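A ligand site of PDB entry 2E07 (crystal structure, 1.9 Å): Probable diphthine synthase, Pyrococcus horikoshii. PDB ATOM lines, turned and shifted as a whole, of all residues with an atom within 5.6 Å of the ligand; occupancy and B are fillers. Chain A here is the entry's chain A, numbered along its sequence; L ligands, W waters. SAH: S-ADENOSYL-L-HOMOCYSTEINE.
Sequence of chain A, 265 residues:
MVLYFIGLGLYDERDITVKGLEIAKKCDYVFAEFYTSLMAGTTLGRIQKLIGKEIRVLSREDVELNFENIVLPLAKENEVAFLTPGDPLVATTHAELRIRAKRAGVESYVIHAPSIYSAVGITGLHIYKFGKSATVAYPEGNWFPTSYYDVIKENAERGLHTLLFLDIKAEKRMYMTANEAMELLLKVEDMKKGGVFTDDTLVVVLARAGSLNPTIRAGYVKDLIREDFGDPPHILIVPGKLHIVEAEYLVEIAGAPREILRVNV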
ATOM      1  N   LEU A  10      19.878 -27.711 -15.117  1.00  0.00           N
ATOM      2  CA  LEU A  10      19.358 -28.592 -14.077  1.00  0.00           C
ATOM      3  C   LEU A  10      20.213 -29.285 -13.045  1.00  0.00           C
ATOM      4  O   LEU A  10      19.859 -29.334 -11.867  1.00  0.00           O
ATOM      5  CB  LEU A  10      18.525 -29.678 -14.751  1.00  0.00           C
ATOM      6  CG  LEU A  10      17.434 -29.250 -15.727  1.00  0.00           C
ATOM      7  CD1 LEU A  10      17.068 -30.416 -16.634  1.00  0.00           C
ATOM      8  CD2 LEU A  10      16.226 -28.760 -14.957  1.00  0.00           C
ATOM      9  N   TYR A  11      21.347 -29.844 -13.471  1.00  0.00           N
ATOM     10  CA  TYR A  11      22.139 -30.662 -12.557  1.00  0.00           C
ATOM     11  C   TYR A  11      23.628 -30.367 -12.410  1.00  0.00           C
ATOM     12  O   TYR A  11      24.132 -30.284 -11.286  1.00  0.00           O
ATOM     13  CB  TYR A  11      21.925 -32.112 -12.992  1.00  0.00           C
ATOM     14  CG  TYR A  11      22.540 -33.160 -12.102  1.00  0.00           C
ATOM     15  CD1 TYR A  11      22.065 -33.383 -10.806  1.00  0.00           C
ATOM     16  CD2 TYR A  11      23.594 -33.939 -12.559  1.00  0.00           C
ATOM     17  CE1 TYR A  11      22.615 -34.370 -10.001  1.00  0.00           C
ATOM     18  CE2 TYR A  11      24.160 -34.940 -11.758  1.00  0.00           C
ATOM     19  CZ  TYR A  11      23.660 -35.148 -10.486  1.00  0.00           C
ATOM     20  OH  TYR A  11      24.209 -36.126  -9.691  1.00  0.00           O
ATOM     21  N   THR A  36      18.122 -20.076  -5.493  1.00  0.00           N
ATOM     22  CA  THR A  36      16.813 -20.350  -6.089  1.00  0.00           C
ATOM     23  C   THR A  36      16.624 -21.830  -6.385  1.00  0.00           C
ATOM     24  O   THR A  36      15.504 -22.305  -6.518  1.00  0.00           O
ATOM     25  CB  THR A  36      16.605 -19.553  -7.394  1.00  0.00           C
ATOM     26  OG1 THR A  36      17.702 -19.791  -8.296  1.00  0.00           O
ATOM     27  CG2 THR A  36      16.500 -18.062  -7.095  1.00  0.00           C
ATOM     28  N   SER A  37      17.719 -22.559  -6.489  1.00  0.00           N
ATOM     29  CA  SER A  37      17.627 -23.985  -6.750  1.00  0.00           C
ATOM     30  C   SER A  37      18.916 -24.692  -6.400  1.00  0.00           C
ATOM     31  O   SER A  37      19.914 -24.059  -6.082  1.00  0.00           O
ATOM     32  CB  SER A  37      17.280 -24.232  -8.225  1.00  0.00           C
ATOM     33  OG  SER A  37      17.020 -25.610  -8.436  1.00  0.00           O
ATOM     34  N   LEU A  38      18.882 -26.019  -6.468  1.00  0.00           N
ATOM     35  CA  LEU A  38      20.053 -26.835  -6.147  1.00  0.00           C
ATOM     36  C   LEU A  38      20.563 -27.628  -7.340  1.00  0.00           C
ATOM     37  O   LEU A  38      19.841 -28.435  -7.929  1.00  0.00           O
ATOM     38  CB  LEU A  38      19.722 -27.812  -5.008  1.00  0.00           C
ATOM     39  CG  LEU A  38      20.822 -28.827  -4.668  1.00  0.00           C
ATOM     40  CD1 LEU A  38      22.033 -28.113  -4.089  1.00  0.00           C
ATOM     41  CD2 LEU A  38      20.286 -29.850  -3.677  1.00  0.00           C
ATOM     42  N   PRO A  85      20.852 -21.150 -11.413  1.00  0.00           N
ATOM     43  CA  PRO A  85      20.567 -22.557 -11.690  1.00  0.00           C
ATOM     44  C   PRO A  85      19.369 -22.586 -12.640  1.00  0.00           C
ATOM     45  O   PRO A  85      18.625 -21.603 -12.731  1.00  0.00           O
ATOM     46  CB  PRO A  85      20.208 -23.117 -10.319  1.00  0.00           C
ATOM     47  CG  PRO A  85      20.973 -22.228  -9.366  1.00  0.00           C
ATOM     48  CD  PRO A  85      20.758 -20.873  -9.974  1.00  0.00           C
ATOM     49  N   GLY A  86      19.191 -23.699 -13.352  1.00  0.00           N
ATOM     50  CA  GLY A  86      18.077 -23.817 -14.275  1.00  0.00           C
ATOM     51  C   GLY A  86      17.987 -22.659 -15.246  1.00  0.00           C
ATOM     52  O   GLY A  86      19.009 -22.217 -15.772  1.00  0.00           O
ATOM     53  N   ASP A  87      16.767 -22.188 -15.505  1.00  0.00           N
ATOM     54  CA  ASP A  87      16.542 -21.038 -16.384  1.00  0.00           C
ATOM     55  C   ASP A  87      16.411 -19.867 -15.423  1.00  0.00           C
ATOM     56  O   ASP A  87      15.676 -19.937 -14.435  1.00  0.00           O
ATOM     57  CB  ASP A  87      15.253 -21.225 -17.194  1.00  0.00           C
ATOM     58  CG  ASP A  87      14.952 -20.040 -18.102  1.00  0.00           C
ATOM     59  OD1 ASP A  87      14.678 -18.942 -17.569  1.00  0.00           O
ATOM     60  OD2 ASP A  87      14.990 -20.214 -19.346  1.00  0.00           O
ATOM     61  N   PRO A  88      17.126 -18.763 -15.694  1.00  0.00           N
ATOM     62  CA  PRO A  88      17.081 -17.583 -14.811  1.00  0.00           C
ATOM     63  C   PRO A  88      15.749 -16.927 -14.514  1.00  0.00           C
ATOM     64  O   PRO A  88      15.609 -16.291 -13.463  1.00  0.00           O
ATOM     65  CB  PRO A  88      18.076 -16.620 -15.469  1.00  0.00           C
ATOM     66  CG  PRO A  88      18.005 -16.995 -16.923  1.00  0.00           C
ATOM     67  CD  PRO A  88      17.950 -18.507 -16.884  1.00  0.00           C
ATOM     68  N   LEU A  89      14.768 -17.080 -15.393  1.00  0.00           N
ATOM     69  CA  LEU A  89      13.477 -16.426 -15.170  1.00  0.00           C
ATOM     70  C   LEU A  89      12.322 -17.351 -14.829  1.00  0.00           C
ATOM     71  O   LEU A  89      11.163 -16.932 -14.846  1.00  0.00           O
ATOM     72  CB  LEU A  89      13.115 -15.593 -16.409  1.00  0.00           C
ATOM     73  CG  LEU A  89      14.157 -14.568 -16.850  1.00  0.00           C
ATOM     74  CD1 LEU A  89      13.647 -13.804 -18.067  1.00  0.00           C
ATOM     75  CD2 LEU A  89      14.437 -13.607 -15.712  1.00  0.00           C
ATOM     76  N   VAL A  90      12.612 -18.605 -14.514  1.00  0.00           N
ATOM     77  CA  VAL A  90      11.569 -19.563 -14.165  1.00  0.00           C
ATOM     78  C   VAL A  90      11.482 -19.806 -12.661  1.00  0.00           C
ATOM     79  O   VAL A  90      12.427 -20.272 -12.039  1.00  0.00           O
ATOM     80  CB  VAL A  90      11.809 -20.919 -14.868  1.00  0.00           C
ATOM     81  CG1 VAL A  90      10.801 -21.959 -14.374  1.00  0.00           C
ATOM     82  CG2 VAL A  90      11.683 -20.753 -16.382  1.00  0.00           C
ATOM     83  N   ALA A  91      10.328 -19.481 -12.086  1.00  0.00           N
ATOM     84  CA  ALA A  91      10.102 -19.678 -10.655  1.00  0.00           C
ATOM     85  C   ALA A  91      11.101 -18.905  -9.794  1.00  0.00           C
ATOM     86  O   ALA A  91      11.506 -19.367  -8.731  1.00  0.00           O
ATOM     87  CB  ALA A  91      10.161 -21.178 -10.316  1.00  0.00           C
ATOM     88  N   THR A  92      11.499 -17.735 -10.283  1.00  0.00           N
ATOM     89  CA  THR A  92      12.330 -16.791  -9.579  1.00  0.00           C
ATOM     90  C   THR A  92      11.709 -15.418  -9.733  1.00  0.00           C
ATOM     91  O   THR A  92      10.761 -15.224 -10.483  1.00  0.00           O
ATOM     92  CB  THR A  92      13.742 -16.783 -10.185  1.00  0.00           C
ATOM     93  OG1 THR A  92      13.752 -16.038 -11.398  1.00  0.00           O
ATOM     94  CG2 THR A  92      14.241 -18.214 -10.464  1.00  0.00           C
ATOM     95  N   PRO A 114      18.122 -25.499 -19.639  1.00  0.00           N
ATOM     96  CA  PRO A 114      17.046 -26.430 -19.280  1.00  0.00           C
ATOM     97  C   PRO A 114      16.441 -26.099 -17.908  1.00  0.00           C
ATOM     98  O   PRO A 114      17.162 -25.784 -16.949  1.00  0.00           O
ATOM     99  CB  PRO A 114      17.729 -27.806 -19.342  1.00  0.00           C
ATOM    100  CG  PRO A 114      19.204 -27.502 -19.284  1.00  0.00           C
ATOM    101  CD  PRO A 114      19.350 -26.210 -20.031  1.00  0.00           C
ATOM    102  N   SER A 115      15.119 -26.163 -17.851  1.00  0.00           N
ATOM    103  CA  SER A 115      14.358 -25.838 -16.642  1.00  0.00           C
ATOM    104  C   SER A 115      13.535 -27.031 -16.163  1.00  0.00           C
ATOM    105  O   SER A 115      13.042 -27.807 -16.975  1.00  0.00           O
ATOM    106  CB  SER A 115      13.418 -24.670 -16.923  1.00  0.00           C
ATOM    107  OG  SER A 115      12.568 -24.404 -15.823  1.00  0.00           O
ATOM    108  N   ILE A 116      13.382 -27.168 -14.857  1.00  0.00           N
ATOM    109  CA  ILE A 116      12.595 -28.274 -14.325  1.00  0.00           C
ATOM    110  C   ILE A 116      11.155 -28.158 -14.836  1.00  0.00           C
ATOM    111  O   ILE A 116      10.447 -29.151 -14.983  1.00  0.00           O
ATOM    112  CB  ILE A 116      12.595 -28.278 -12.781  1.00  0.00           C
ATOM    113  CG1 ILE A 116      11.927 -29.565 -12.287  1.00  0.00           C
ATOM    114  CG2 ILE A 116      11.871 -27.043 -12.249  1.00  0.00           C
ATOM    115  CD1 ILE A 116      12.698 -30.821 -12.645  1.00  0.00           C
ATOM    116  N   TYR A 117      10.730 -26.926 -15.123  1.00  0.00           N
ATOM    117  CA  TYR A 117       9.382 -26.674 -15.607  1.00  0.00           C
ATOM    118  C   TYR A 117       9.066 -27.460 -16.890  1.00  0.00           C
ATOM    119  O   TYR A 117       7.936 -27.915 -17.072  1.00  0.00           O
ATOM    120  CB  TYR A 117       9.186 -25.170 -15.833  1.00  0.00           C
ATOM    121  CG  TYR A 117       7.791 -24.761 -16.239  1.00  0.00           C
ATOM    122  CD1 TYR A 117       6.707 -24.928 -15.379  1.00  0.00           C
ATOM    123  CD2 TYR A 117       7.553 -24.170 -17.486  1.00  0.00           C
ATOM    124  CE1 TYR A 117       5.429 -24.521 -15.746  1.00  0.00           C
ATOM    125  CE2 TYR A 117       6.287 -23.756 -17.858  1.00  0.00           C
ATOM    126  CZ  TYR A 117       5.227 -23.927 -16.983  1.00  0.00           C
ATOM    127  OH  TYR A 117       3.969 -23.505 -17.367  1.00  0.00           O
ATOM    128  N   LEU A 164       4.497 -29.356  -8.605  1.00  0.00           N
ATOM    129  CA  LEU A 164       4.743 -28.760  -7.304  1.00  0.00           C
ATOM    130  C   LEU A 164       6.221 -28.559  -7.051  1.00  0.00           C
ATOM    131  O   LEU A 164       6.975 -29.517  -6.837  1.00  0.00           O
ATOM    132  CB  LEU A 164       4.158 -29.644  -6.193  1.00  0.00           C
ATOM    133  CG  LEU A 164       2.646 -29.878  -6.249  1.00  0.00           C
ATOM    134  CD1 LEU A 164       2.254 -30.973  -5.260  1.00  0.00           C
ATOM    135  CD2 LEU A 164       1.911 -28.581  -5.943  1.00  0.00           C
ATOM    136  N   PHE A 165       6.659 -27.304  -7.113  1.00  0.00           N
ATOM    137  CA  PHE A 165       8.047 -26.971  -6.831  1.00  0.00           C
ATOM    138  C   PHE A 165       8.144 -27.202  -5.329  1.00  0.00           C
ATOM    139  O   PHE A 165       7.168 -26.989  -4.611  1.00  0.00           O
ATOM    140  CB  PHE A 165       8.297 -25.483  -7.127  1.00  0.00           C
ATOM    141  CG  PHE A 165       8.221 -25.131  -8.581  1.00  0.00           C
ATOM    142  CD1 PHE A 165       9.290 -25.370  -9.432  1.00  0.00           C
ATOM    143  CD2 PHE A 165       7.061 -24.563  -9.107  1.00  0.00           C
ATOM    144  CE1 PHE A 165       9.219 -25.034 -10.783  1.00  0.00           C
ATOM    145  CE2 PHE A 165       6.978 -24.225 -10.465  1.00  0.00           C
ATOM    146  CZ  PHE A 165       8.062 -24.467 -11.300  1.00  0.00           C
ATOM    147  N   LEU A 166       9.303 -27.659  -4.854  1.00  0.00           N
ATOM    148  CA  LEU A 166       9.473 -27.909  -3.416  1.00  0.00           C
ATOM    149  C   LEU A 166      10.392 -26.855  -2.788  1.00  0.00           C
ATOM    150  O   LEU A 166      11.310 -26.345  -3.429  1.00  0.00           O
ATOM    151  CB  LEU A 166      10.032 -29.317  -3.192  1.00  0.00           C
ATOM    152  CG  LEU A 166       9.138 -30.415  -3.775  1.00  0.00           C
ATOM    153  CD1 LEU A 166       9.647 -31.770  -3.327  1.00  0.00           C
ATOM    154  CD2 LEU A 166       7.687 -30.217  -3.312  1.00  0.00           C
ATOM    155  N   ASP A 167      10.134 -26.542  -1.530  1.00  0.00           N
ATOM    156  CA  ASP A 167      10.888 -25.500  -0.833  1.00  0.00           C
ATOM    157  C   ASP A 167      12.393 -25.752  -0.718  1.00  0.00           C
ATOM    158  O   ASP A 167      12.861 -26.887  -0.755  1.00  0.00           O
ATOM    159  CB  ASP A 167      10.308 -25.296   0.572  1.00  0.00           C
ATOM    160  CG  ASP A 167      10.458 -23.860   1.056  1.00  0.00           C
ATOM    161  OD1 ASP A 167      11.093 -23.048   0.346  1.00  0.00           O
ATOM    162  OD2 ASP A 167       9.930 -23.529   2.145  1.00  0.00           O
ATOM    163  N   ILE A 168      13.130 -24.654  -0.589  1.00  0.00           N
ATOM    164  CA  ILE A 168      14.579 -24.719  -0.445  1.00  0.00           C
ATOM    165  C   ILE A 168      15.080 -23.573   0.433  1.00  0.00           C
ATOM    166  O   ILE A 168      14.700 -22.417   0.247  1.00  0.00           O
ATOM    167  CB  ILE A 168      15.295 -24.644  -1.824  1.00  0.00           C
ATOM    168  CG1 ILE A 168      16.795 -24.471  -1.619  1.00  0.00           C
ATOM    169  CG2 ILE A 168      14.721 -23.499  -2.651  1.00  0.00           C
ATOM    170  CD1 ILE A 168      17.610 -24.402  -2.912  1.00  0.00           C
ATOM    171  N   LEU A 206      10.055 -36.798  -9.361  1.00  0.00           N
ATOM    172  CA  LEU A 206      11.195 -36.666 -10.259  1.00  0.00           C
ATOM    173  C   LEU A 206      12.306 -36.072  -9.423  1.00  0.00           C
ATOM    174  O   LEU A 206      12.187 -34.946  -8.926  1.00  0.00           O
ATOM    175  CB  LEU A 206      10.871 -35.736 -11.445  1.00  0.00           C
ATOM    176  CG  LEU A 206      12.077 -35.444 -12.351  1.00  0.00           C
ATOM    177  CD1 LEU A 206      12.648 -36.750 -12.912  1.00  0.00           C
ATOM    178  CD2 LEU A 206      11.649 -34.520 -13.485  1.00  0.00           C
ATOM    179  N   ALA A 207      13.387 -36.826  -9.272  1.00  0.00           N
ATOM    180  CA  ALA A 207      14.516 -36.371  -8.485  1.00  0.00           C
ATOM    181  C   ALA A 207      15.784 -36.231  -9.317  1.00  0.00           C
ATOM    182  O   ALA A 207      16.131 -37.132 -10.078  1.00  0.00           O
ATOM    183  CB  ALA A 207      14.755 -37.324  -7.316  1.00  0.00           C
ATOM    184  N   ARG A 208      16.454 -35.106  -9.147  1.00  0.00           N
ATOM    185  CA  ARG A 208      17.710 -34.825  -9.838  1.00  0.00           C
ATOM    186  C   ARG A 208      17.582 -34.854 -11.355  1.00  0.00           C
ATOM    187  O   ARG A 208      18.371 -35.506 -12.044  1.00  0.00           O
ATOM    188  CB  ARG A 208      18.805 -35.791  -9.371  1.00  0.00           C
ATOM    189  CG  ARG A 208      19.053 -35.747  -7.859  1.00  0.00           C
ATOM    190  CD  ARG A 208      20.108 -36.788  -7.433  1.00  0.00           C
ATOM    191  NE  ARG A 208      19.755 -38.110  -7.929  1.00  0.00           N
ATOM    192  CZ  ARG A 208      18.723 -38.830  -7.475  1.00  0.00           C
ATOM    193  NH1 ARG A 208      17.940 -38.360  -6.519  1.00  0.00           N
ATOM    194  NH2 ARG A 208      18.460 -40.010  -8.028  1.00  0.00           N
ATOM    195  N   ALA A 209      16.567 -34.163 -11.880  1.00  0.00           N
ATOM    196  CA  ALA A 209      16.393 -34.107 -13.330  1.00  0.00           C
ATOM    197  C   ALA A 209      17.674 -33.464 -13.857  1.00  0.00           C
ATOM    198  O   ALA A 209      18.279 -32.647 -13.171  1.00  0.00           O
ATOM    199  CB  ALA A 209      15.184 -33.234 -13.681  1.00  0.00           C
ATOM    200  N   GLY A 210      18.073 -33.835 -15.065  1.00  0.00           N
ATOM    201  CA  GLY A 210      19.296 -33.273 -15.618  1.00  0.00           C
ATOM    202  C   GLY A 210      20.429 -34.275 -15.496  1.00  0.00           C
ATOM    203  O   GLY A 210      21.338 -34.306 -16.328  1.00  0.00           O
ATOM    204  N   PRO A 233      17.796 -32.193  -5.618  1.00  0.00           N
ATOM    205  CA  PRO A 233      16.434 -31.661  -5.469  1.00  0.00           C
ATOM    206  C   PRO A 233      15.351 -32.613  -5.974  1.00  0.00           C
ATOM    207  O   PRO A 233      15.597 -33.476  -6.819  1.00  0.00           O
ATOM    208  CB  PRO A 233      16.487 -30.372  -6.272  1.00  0.00           C
ATOM    209  CG  PRO A 233      17.373 -30.742  -7.425  1.00  0.00           C
ATOM    210  CD  PRO A 233      18.492 -31.539  -6.755  1.00  0.00           C
ATOM    211  N   HIS A 234      14.153 -32.444  -5.430  1.00  0.00           N
ATOM    212  CA  HIS A 234      12.995 -33.250  -5.796  1.00  0.00           C
ATOM    213  C   HIS A 234      11.860 -32.346  -6.242  1.00  0.00           C
ATOM    214  O   HIS A 234      11.785 -31.184  -5.840  1.00  0.00           O
ATOM    215  CB  HIS A 234      12.445 -34.046  -4.600  1.00  0.00           C
ATOM    216  CG  HIS A 234      13.364 -35.115  -4.072  1.00  0.00           C
ATOM    217  ND1 HIS A 234      12.998 -35.936  -3.024  1.00  0.00           N
ATOM    218  CD2 HIS A 234      14.607 -35.500  -4.444  1.00  0.00           C
ATOM    219  CE1 HIS A 234      13.982 -36.777  -2.773  1.00  0.00           C
ATOM    220  NE2 HIS A 234      14.970 -36.538  -3.615  1.00  0.00           N
ATOM    221  N   ILE A 235      10.980 -32.887  -7.062  1.00  0.00           N
ATOM    222  CA  ILE A 235       9.807 -32.157  -7.468  1.00  0.00           C
ATOM    223  C   ILE A 235       8.663 -33.168  -7.381  1.00  0.00           C
ATOM    224  O   ILE A 235       8.880 -34.362  -7.606  1.00  0.00           O
ATOM    225  CB  ILE A 235       9.957 -31.554  -8.892  1.00  0.00           C
ATOM    226  CG1 ILE A 235       9.070 -30.318  -9.010  1.00  0.00           C
ATOM    227  CG2 ILE A 235       9.608 -32.578  -9.959  1.00  0.00           C
ATOM    228  CD1 ILE A 235       9.536 -29.312 -10.043  1.00  0.00           C
HETATM  229  N   SAH L   1      14.712 -21.507 -12.282  1.00  0.00           N
HETATM  230  CA  SAH L   1      14.730 -22.960 -11.794  1.00  0.00           C
HETATM  231  CB  SAH L   1      13.730 -23.339 -10.741  1.00  0.00           C
HETATM  232  CG  SAH L   1      13.730 -22.586  -9.418  1.00  0.00           C
HETATM  233  SD  SAH L   1      12.520 -23.431  -8.319  1.00  0.00           S
HETATM  234  C   SAH L   1      14.556 -23.868 -13.078  1.00  0.00           C
HETATM  235  O   SAH L   1      14.425 -23.313 -14.190  1.00  0.00           O
HETATM  236  OXT SAH L   1      14.560 -25.139 -12.886  1.00  0.00           O
HETATM  237  C5' SAH L   1      13.596 -24.560  -7.504  1.00  0.00           C
HETATM  238  C4' SAH L   1      12.829 -25.908  -7.221  1.00  0.00           C
HETATM  239  O4' SAH L   1      12.562 -26.539  -8.495  1.00  0.00           O
HETATM  240  C3' SAH L   1      13.576 -26.895  -6.401  1.00  0.00           C
HETATM  241  O3' SAH L   1      13.385 -26.641  -5.017  1.00  0.00           O
HETATM  242  C2' SAH L   1      13.001 -28.232  -6.915  1.00  0.00           C
HETATM  243  O2' SAH L   1      11.765 -28.560  -6.261  1.00  0.00           O
HETATM  244  C1' SAH L   1      12.854 -28.011  -8.433  1.00  0.00           C
HETATM  245  N9  SAH L   1      13.969 -28.305  -9.162  1.00  0.00           N
HETATM  246  C8  SAH L   1      14.978 -27.566  -9.744  1.00  0.00           C
HETATM  247  N7  SAH L   1      15.882 -28.261 -10.374  1.00  0.00           N
HETATM  248  C5  SAH L   1      15.475 -29.609 -10.208  1.00  0.00           C
HETATM  249  C6  SAH L   1      16.048 -30.859 -10.664  1.00  0.00           C
HETATM  250  N6  SAH L   1      17.181 -30.942 -11.386  1.00  0.00           N
HETATM  251  N1  SAH L   1      15.343 -31.991 -10.303  1.00  0.00           N
HETATM  252  C2  SAH L   1      14.200 -31.957  -9.578  1.00  0.00           C
HETATM  253  N3  SAH L   1      13.629 -30.790  -9.124  1.00  0.00           N
HETATM  254  C4  SAH L   1      14.313 -29.663  -9.479  1.00  0.00           C
HETATM  255  O   HOH W   1      16.738 -20.963 -10.632  1.00  0.00           O
HETATM  256  O   HOH W   2      14.685 -28.034  -2.822  1.00  0.00           O
HETATM  257  O   HOH W   3      17.092 -26.256 -12.210  1.00  0.00           O
HETATM  258  O   HOH W   4      18.732 -26.516 -10.456  1.00  0.00           O
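The side-chain hydroxyl (OG) of Ser 115 sits at hydrogen-bond distance from an oxygen (O) of the ligand (2.7 Å).
An oxygen (O2') of the ligand is in hydrogen-bond range of the backbone NH (N) of Leu 166, at 3.0 Å.
N7 of the ligand sits close to OG of Ser 37, 3.5 Å away.
A nitrogen (N) of the ligand sits at hydrogen-bond distance from the backbone carbonyl oxygen of Val 90 (2.6 Å).
The backbone NH of Asp 87 sits at hydrogen-bond distance from an oxygen (O) of the ligand (2.9 Å).
O of Leu 10 sits at hydrogen-bond distance from N6 of the ligand.
The backbone carbonyl oxygen (O) of Leu 166 sits at hydrogen-bond distance from an oxygen (O3') of the ligand, 2.6 Å away.
A nitrogen (N6) of the ligand sits at hydrogen-bond distance from the backbone carbonyl oxygen (O) of Ala 209, 2.7 Å away.
An oxygen (OXT) of the ligand lies within hydrogen-bond range of the backbone NH of Ile 116.
A nitrogen (N1) of the ligand sits at hydrogen-bond distance from the backbone NH of Ala 209 (3.0 Å).
O2' of the ligand sits at hydrogen-bond distance from O of His 234, at 2.7 Å.
N of the ligand lies within hydrogen-bond range of O of Asp 87, at 2.8 Å.
The backbone NH of Arg 208 lies within hydrogen-bond range of the backbone carbonyl oxygen of Pro 233, at 3.0 Å.
The side-chain carboxylate (OD1) of Asp 87 sits at hydrogen-bond distance from the backbone NH (N) of Leu 89 (2.9 Å).
The backbone carbonyl oxygen (O) of Leu 206 lies within hydrogen-bond range of the backbone NH (N) of Ile 235.
N of Tyr 117 sits close to OG of Ser 115, at 3.2 Å.
O of Pro 88 is in hydrogen-bond range of OG1 of Thr 92 (2.8 Å).
SD of the ligand lies close to O of Thr 36 (3.7 Å).
Merely in contact with the ligand: Pro 233, Arg 208, Phe 165, Leu 206, Gly 86, Ile 235, Thr 92, Ala 91 and Pro 85.
Hydrophobic or aromatic side chains within 4 Å of the ligand: Leu 10, Val 90, Ala 91, Ile 116, Phe 165, Leu 166, Ala 209, Pro 233 and Ile 235.
Within 4 Å of the ligand: Leu 10, Thr 36, Ser 37, Pro 85, Gly 86, Asp 87, Val 90, Ala 91, Thr 92, Ser 115, Ile 116, Phe 165, Leu 166, Leu 206, Arg 208, Ala 209, Pro 233, His 234 and Ile 235.
Along chain A the residues within 4 Å of the ligand span positions 10 to 235.
The nearest printed residue that does not touch the ligand is Ile 168 (4.2 Å).
Water W1 lies within hydrogen-bond range of N of the ligand (2.7 Å), OG1 of Thr 36 (2.8 Å) and O of Pro 85 (2.9 Å).
Water W3 lies within hydrogen-bond range of OXT of the ligand (2.8 Å) and N of Gly 86 (3.5 Å).
Water W2 lies within hydrogen-bond range of an oxygen (O3') of the ligand (2.9 Å) and the backbone carbonyl oxygen of Asp 167 (3.0 Å).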
